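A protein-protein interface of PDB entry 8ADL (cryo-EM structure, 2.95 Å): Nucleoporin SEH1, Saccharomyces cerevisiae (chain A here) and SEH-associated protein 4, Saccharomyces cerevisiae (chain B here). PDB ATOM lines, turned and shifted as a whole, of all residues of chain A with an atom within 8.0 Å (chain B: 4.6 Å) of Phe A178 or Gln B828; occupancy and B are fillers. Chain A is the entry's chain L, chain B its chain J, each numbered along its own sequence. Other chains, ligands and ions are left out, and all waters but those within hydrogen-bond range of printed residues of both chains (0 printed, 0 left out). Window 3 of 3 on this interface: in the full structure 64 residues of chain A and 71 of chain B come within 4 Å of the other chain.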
ATOM      1  N   HIS A 120      -0.858  23.501  -3.827  1.00  0.00           N
ATOM      2  CA  HIS A 120      -1.611  22.324  -4.235  1.00  0.00           C
ATOM      3  C   HIS A 120      -0.869  21.471  -5.255  1.00  0.00           C
ATOM      4  O   HIS A 120      -1.290  20.337  -5.510  1.00  0.00           O
ATOM      5  CB  HIS A 120      -2.970  22.736  -4.806  1.00  0.00           C
ATOM      6  CG  HIS A 120      -2.880  23.514  -6.081  1.00  0.00           C
ATOM      7  ND1 HIS A 120      -2.789  24.888  -6.109  1.00  0.00           N
ATOM      8  CD2 HIS A 120      -2.882  23.111  -7.373  1.00  0.00           C
ATOM      9  CE1 HIS A 120      -2.729  25.297  -7.364  1.00  0.00           C
ATOM     10  NE2 HIS A 120      -2.783  24.238  -8.150  1.00  0.00           N
ATOM     11  N   CYS A 174       0.394  29.897 -12.056  1.00  0.00           N
ATOM     12  CA  CYS A 174      -1.033  30.160 -11.996  1.00  0.00           C
ATOM     13  C   CYS A 174      -1.536  29.739 -10.626  1.00  0.00           C
ATOM     14  O   CYS A 174      -1.547  28.535 -10.327  1.00  0.00           O
ATOM     15  CB  CYS A 174      -1.771  29.399 -13.096  1.00  0.00           C
ATOM     16  SG  CYS A 174      -3.568  29.384 -12.923  1.00  0.00           S
ATOM     17  N   PRO A 175      -1.958  30.674  -9.760  1.00  0.00           N
ATOM     18  CA  PRO A 175      -2.375  30.329  -8.396  1.00  0.00           C
ATOM     19  C   PRO A 175      -3.834  29.894  -8.303  1.00  0.00           C
ATOM     20  O   PRO A 175      -4.603  30.390  -7.471  1.00  0.00           O
ATOM     21  CB  PRO A 175      -2.121  31.630  -7.629  1.00  0.00           C
ATOM     22  CG  PRO A 175      -2.368  32.690  -8.640  1.00  0.00           C
ATOM     23  CD  PRO A 175      -1.960  32.129  -9.979  1.00  0.00           C
ATOM     24  N   SER A 176      -4.230  28.958  -9.162  1.00  0.00           N
ATOM     25  CA  SER A 176      -5.581  28.419  -9.171  1.00  0.00           C
ATOM     26  C   SER A 176      -5.492  26.907  -9.057  1.00  0.00           C
ATOM     27  O   SER A 176      -4.833  26.259  -9.876  1.00  0.00           O
ATOM     28  CB  SER A 176      -6.329  28.821 -10.444  1.00  0.00           C
ATOM     29  OG  SER A 176      -5.714  28.262 -11.592  1.00  0.00           O
ATOM     30  N   ARG A 177      -6.152  26.348  -8.047  1.00  0.00           N
ATOM     31  CA  ARG A 177      -6.188  24.908  -7.843  1.00  0.00           C
ATOM     32  C   ARG A 177      -7.350  24.250  -8.569  1.00  0.00           C
ATOM     33  O   ARG A 177      -7.563  23.043  -8.414  1.00  0.00           O
ATOM     34  CB  ARG A 177      -6.247  24.591  -6.348  1.00  0.00           C
ATOM     35  CG  ARG A 177      -7.081  25.564  -5.535  1.00  0.00           C
ATOM     36  CD  ARG A 177      -6.922  25.293  -4.052  1.00  0.00           C
ATOM     37  NE  ARG A 177      -7.363  23.951  -3.693  1.00  0.00           N
ATOM     38  CZ  ARG A 177      -7.112  23.368  -2.529  1.00  0.00           C
ATOM     39  NH1 ARG A 177      -6.422  23.983  -1.583  1.00  0.00           N
ATOM     40  NH2 ARG A 177      -7.566  22.137  -2.309  1.00  0.00           N
ATOM     41  N   PHE A 178      -8.101  25.018  -9.356  1.00  0.00           N
ATOM     42  CA  PHE A 178      -9.242  24.519 -10.110  1.00  0.00           C
ATOM     43  C   PHE A 178      -8.982  24.549 -11.609  1.00  0.00           C
ATOM     44  O   PHE A 178      -9.923  24.472 -12.406  1.00  0.00           O
ATOM     45  CB  PHE A 178     -10.485  25.327  -9.746  1.00  0.00           C
ATOM     46  CG  PHE A 178     -10.745  25.373  -8.273  1.00  0.00           C
ATOM     47  CD1 PHE A 178     -11.394  24.327  -7.640  1.00  0.00           C
ATOM     48  CD2 PHE A 178     -10.306  26.445  -7.513  1.00  0.00           C
ATOM     49  CE1 PHE A 178     -11.621  24.358  -6.280  1.00  0.00           C
ATOM     50  CE2 PHE A 178     -10.522  26.478  -6.154  1.00  0.00           C
ATOM     51  CZ  PHE A 178     -11.186  25.437  -5.537  1.00  0.00           C
ATOM     52  N   SER A 179      -7.721  24.663 -11.996  1.00  0.00           N
ATOM     53  CA  SER A 179      -7.282  24.701 -13.379  1.00  0.00           C
ATOM     54  C   SER A 179      -6.029  23.845 -13.475  1.00  0.00           C
ATOM     55  O   SER A 179      -5.362  23.606 -12.461  1.00  0.00           O
ATOM     56  CB  SER A 179      -7.004  26.148 -13.813  1.00  0.00           C
ATOM     57  OG  SER A 179      -6.655  26.249 -15.180  1.00  0.00           O
ATOM     58  N   PRO A 180      -5.702  23.337 -14.666  1.00  0.00           N
ATOM     59  CA  PRO A 180      -4.452  22.584 -14.825  1.00  0.00           C
ATOM     60  C   PRO A 180      -3.221  23.442 -14.566  1.00  0.00           C
ATOM     61  O   PRO A 180      -3.258  24.674 -14.618  1.00  0.00           O
ATOM     62  CB  PRO A 180      -4.507  22.113 -16.281  1.00  0.00           C
ATOM     63  CG  PRO A 180      -5.951  22.006 -16.568  1.00  0.00           C
ATOM     64  CD  PRO A 180      -6.615  23.110 -15.800  1.00  0.00           C
ATOM     65  N   GLU A 181      -2.119  22.754 -14.268  1.00  0.00           N
ATOM     66  CA  GLU A 181      -0.865  23.404 -13.905  1.00  0.00           C
ATOM     67  C   GLU A 181      -0.301  24.214 -15.064  1.00  0.00           C
ATOM     68  O   GLU A 181      -0.027  23.673 -16.138  1.00  0.00           O
ATOM     69  CB  GLU A 181       0.146  22.349 -13.455  1.00  0.00           C
ATOM     70  CG  GLU A 181       1.587  22.829 -13.425  1.00  0.00           C
ATOM     71  CD  GLU A 181       2.549  21.745 -12.984  1.00  0.00           C
ATOM     72  OE1 GLU A 181       2.105  20.800 -12.300  1.00  0.00           O
ATOM     73  OE2 GLU A 181       3.746  21.837 -13.324  1.00  0.00           O
ATOM     74  N   LYS A 182      -0.142  25.516 -14.845  1.00  0.00           N
ATOM     75  CA  LYS A 182       0.365  26.433 -15.852  1.00  0.00           C
ATOM     76  C   LYS A 182       1.546  27.209 -15.290  1.00  0.00           C
ATOM     77  O   LYS A 182       1.724  27.323 -14.076  1.00  0.00           O
ATOM     78  CB  LYS A 182      -0.707  27.411 -16.348  1.00  0.00           C
ATOM     79  CG  LYS A 182      -1.908  26.759 -17.001  1.00  0.00           C
ATOM     80  CD  LYS A 182      -2.903  27.808 -17.457  1.00  0.00           C
ATOM     81  CE  LYS A 182      -4.227  27.178 -17.820  1.00  0.00           C
ATOM     82  NZ  LYS A 182      -4.879  26.586 -16.632  1.00  0.00           N
ATOM     83  N   SER A 223      -6.351  34.221  -8.833  1.00  0.00           N
ATOM     84  CA  SER A 223      -7.654  33.680  -9.208  1.00  0.00           C
ATOM     85  C   SER A 223      -8.616  33.887  -8.048  1.00  0.00           C
ATOM     86  O   SER A 223      -8.625  33.118  -7.084  1.00  0.00           O
ATOM     87  CB  SER A 223      -7.534  32.205  -9.572  1.00  0.00           C
ATOM     88  OG  SER A 223      -8.797  31.566  -9.534  1.00  0.00           O
ATOM     89  N   GLY A 225     -11.938  33.917  -8.443  1.00  0.00           N
ATOM     90  CA  GLY A 225     -13.183  33.222  -8.703  1.00  0.00           C
ATOM     91  C   GLY A 225     -13.799  33.617 -10.027  1.00  0.00           C
ATOM     92  O   GLY A 225     -14.799  33.034 -10.458  1.00  0.00           O
ATOM     93  N   GLU A 247     -10.244  29.862 -20.310  1.00  0.00           N
ATOM     94  CA  GLU A 247      -9.990  28.435 -20.431  1.00  0.00           C
ATOM     95  C   GLU A 247     -11.305  27.671 -20.442  1.00  0.00           C
ATOM     96  O   GLU A 247     -12.222  27.981 -19.675  1.00  0.00           O
ATOM     97  CB  GLU A 247      -9.108  27.936 -19.283  1.00  0.00           C
ATOM     98  CG  GLU A 247      -8.464  26.589 -19.538  1.00  0.00           C
ATOM     99  CD  GLU A 247      -7.833  26.006 -18.291  1.00  0.00           C
ATOM    100  OE1 GLU A 247      -8.173  26.467 -17.182  1.00  0.00           O
ATOM    101  OE2 GLU A 247      -6.997  25.088 -18.423  1.00  0.00           O
ATOM    102  N   GLN A 289      -5.072  19.156 -21.138  1.00  0.00           N
ATOM    103  CA  GLN A 289      -6.339  18.925 -20.450  1.00  0.00           C
ATOM    104  C   GLN A 289      -7.444  19.823 -20.995  1.00  0.00           C
ATOM    105  O   GLN A 289      -8.591  19.383 -21.139  1.00  0.00           O
ATOM    106  CB  GLN A 289      -6.165  19.144 -18.947  1.00  0.00           C
ATOM    107  CG  GLN A 289      -7.159  18.379 -18.089  1.00  0.00           C
ATOM    108  CD  GLN A 289      -6.743  18.316 -16.632  1.00  0.00           C
ATOM    109  OE1 GLN A 289      -5.598  18.612 -16.289  1.00  0.00           O
ATOM    110  NE2 GLN A 289      -7.674  17.932 -15.766  1.00  0.00           N
ATOM    111  N   SER A 290      -7.123  21.076 -21.307  1.00  0.00           N
ATOM    112  CA  SER A 290      -8.119  22.017 -21.804  1.00  0.00           C
ATOM    113  C   SER A 290      -7.415  23.111 -22.591  1.00  0.00           C
ATOM    114  O   SER A 290      -6.406  23.653 -22.129  1.00  0.00           O
ATOM    115  CB  SER A 290      -8.926  22.624 -20.652  1.00  0.00           C
ATOM    116  OG  SER A 290      -8.068  23.173 -19.668  1.00  0.00           O
ATOM    117  N   ASP B 827     -21.878  22.915  -7.276  1.00  0.00           N
ATOM    118  CA  ASP B 827     -21.243  23.589  -8.401  1.00  0.00           C
ATOM    119  C   ASP B 827     -19.811  23.957  -8.036  1.00  0.00           C
ATOM    120  O   ASP B 827     -19.467  24.119  -6.863  1.00  0.00           O
ATOM    121  CB  ASP B 827     -22.019  24.842  -8.824  1.00  0.00           C
ATOM    122  CG  ASP B 827     -21.974  25.930  -7.780  1.00  0.00           C
ATOM    123  OD1 ASP B 827     -22.532  25.723  -6.681  1.00  0.00           O
ATOM    124  OD2 ASP B 827     -21.377  26.991  -8.056  1.00  0.00           O
ATOM    125  N   GLN B 828     -18.976  24.089  -9.069  1.00  0.00           N
ATOM    126  CA  GLN B 828     -17.549  24.323  -8.870  1.00  0.00           C
ATOM    127  C   GLN B 828     -17.235  25.767  -8.494  1.00  0.00           C
ATOM    128  O   GLN B 828     -16.216  26.020  -7.837  1.00  0.00           O
ATOM    129  CB  GLN B 828     -16.779  23.938 -10.135  1.00  0.00           C
ATOM    130  CG  GLN B 828     -15.307  23.635  -9.909  1.00  0.00           C
ATOM    131  CD  GLN B 828     -14.551  23.421 -11.206  1.00  0.00           C
ATOM    132  OE1 GLN B 828     -15.107  23.575 -12.294  1.00  0.00           O
ATOM    133  NE2 GLN B 828     -13.277  23.065 -11.097  1.00  0.00           N
ATOM    134  N   ARG B 829     -18.079  26.717  -8.908  1.00  0.00           N
ATOM    135  CA  ARG B 829     -17.817  28.130  -8.642  1.00  0.00           C
ATOM    136  C   ARG B 829     -17.864  28.443  -7.151  1.00  0.00           C
ATOM    137  O   ARG B 829     -17.041  29.216  -6.646  1.00  0.00           O
ATOM    138  CB  ARG B 829     -18.817  28.998  -9.402  1.00  0.00           C
ATOM    139  CG  ARG B 829     -18.849  28.747 -10.898  1.00  0.00           C
ATOM    140  CD  ARG B 829     -19.974  29.526 -11.556  1.00  0.00           C
ATOM    141  NE  ARG B 829     -21.282  28.959 -11.249  1.00  0.00           N
ATOM    142  CZ  ARG B 829     -22.375  29.165 -11.971  1.00  0.00           C
ATOM    143  NH1 ARG B 829     -22.356  29.925 -13.053  1.00  0.00           N
ATOM    144  NH2 ARG B 829     -23.516  28.594 -11.595  1.00  0.00           N
ATOM    145  N   VAL B 830     -18.812  27.842  -6.430  1.00  0.00           N
ATOM    146  CA  VAL B 830     -18.903  28.064  -4.991  1.00  0.00           C
ATOM    147  C   VAL B 830     -17.714  27.437  -4.276  1.00  0.00           C
ATOM    148  O   VAL B 830     -17.189  28.001  -3.309  1.00  0.00           O
ATOM    149  CB  VAL B 830     -20.248  27.529  -4.465  1.00  0.00           C
ATOM    150  CG1 VAL B 830     -20.290  27.546  -2.947  1.00  0.00           C
ATOM    151  CG2 VAL B 830     -21.383  28.358  -5.030  1.00  0.00           C
ATOM    152  N   ASP B 831     -17.255  26.276  -4.753  1.00  0.00           N
ATOM    153  CA  ASP B 831     -16.056  25.660  -4.192  1.00  0.00           C
ATOM    154  C   ASP B 831     -14.833  26.545  -4.404  1.00  0.00           C
ATOM    155  O   ASP B 831     -13.997  26.690  -3.501  1.00  0.00           O
ATOM    156  CB  ASP B 831     -15.836  24.281  -4.811  1.00  0.00           C
ATOM    157  CG  ASP B 831     -17.049  23.386  -4.679  1.00  0.00           C
ATOM    158  OD1 ASP B 831     -18.021  23.796  -4.011  1.00  0.00           O
ATOM    159  OD2 ASP B 831     -17.034  22.273  -5.244  1.00  0.00           O
ATOM    160  N   GLU B 832     -14.730  27.161  -5.586  1.00  0.00           N
ATOM    161  CA  GLU B 832     -13.648  28.105  -5.851  1.00  0.00           C
ATOM    162  C   GLU B 832     -13.721  29.314  -4.928  1.00  0.00           C
ATOM    163  O   GLU B 832     -12.696  29.759  -4.397  1.00  0.00           O
ATOM    164  CB  GLU B 832     -13.683  28.546  -7.314  1.00  0.00           C
ATOM    165  CG  GLU B 832     -12.492  29.386  -7.732  1.00  0.00           C
ATOM    166  CD  GLU B 832     -12.444  29.622  -9.227  1.00  0.00           C
ATOM    167  OE1 GLU B 832     -13.371  29.170  -9.931  1.00  0.00           O
ATOM    168  OE2 GLU B 832     -11.479  30.259  -9.699  1.00  0.00           O
ATOM    169  N   GLN B 835     -12.737  28.184  -1.295  1.00  0.00           N
ATOM    170  CA  GLN B 835     -11.297  27.973  -1.191  1.00  0.00           C
ATOM    171  C   GLN B 835     -10.531  29.289  -1.246  1.00  0.00           C
ATOM    172  O   GLN B 835      -9.555  29.475  -0.509  1.00  0.00           O
ATOM    173  CB  GLN B 835     -10.825  27.027  -2.293  1.00  0.00           C
ATOM    174  CG  GLN B 835     -11.037  25.558  -1.967  1.00  0.00           C
ATOM    175  CD  GLN B 835     -10.236  25.103  -0.766  1.00  0.00           C
ATOM    176  OE1 GLN B 835      -9.056  25.426  -0.631  1.00  0.00           O
ATOM    177  NE2 GLN B 835     -10.875  24.343   0.116  1.00  0.00           N
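Among the printed residues, pairs that only touch across the chains: Phe A178 with Gln B828 (3.8 Å), Phe A178 with Asp B831 (3.7 Å), Phe A178 with Glu B832 (3.5 Å), Phe A178 with Gln B835 (3.6 Å) and Gly A225 with Glu B832 (3.6 Å).
Printed residues of chain B within 4 Å of Arg A177: Gln B835 (3.2 Å). Phe A178 touches four residues of chain B. Of the printed residues of chain B, Ser A223 touches Glu B832 (3.0 Å). Printed residues of chain A within 4 Å of Glu B832: Phe A178 (3.5 Å), Ser A223 (3.0 Å) and Gly A225 (3.6 Å). Of the printed residues of chain A, Gln B835 touches Arg A177 (3.2 Å) and Phe A178 (3.6 Å). The nearest printed residue of chain B that does not touch Phe A178 is Val B830 (6.9 Å). The nearest residue of chain A that does not touch Gln B828 is Ser A179 (5.9 Å). The nearest printed residue of chain B that does not touch Ser A223 is Gln B835 (7.2 Å).
NH1 of Arg A177 lies within hydrogen-bond range of OE1 of Gln B835 (3.2 Å). The side-chain carboxylate (OE2) of Glu B832 is in hydrogen-bond range of the side-chain hydroxyl (OG) of Ser A223 (3.0 Å).
Printed residues of chain B that touch a printed residue of chain A: Gln B828, Asp B831, Glu B832 and Gln B835. Among the printed residues, 7 pairs touch across the chains. Among the printed residues, no Asp or Glu carboxylate lies within 4 Å of a Lys or Arg side-chain nitrogen of the other chain.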
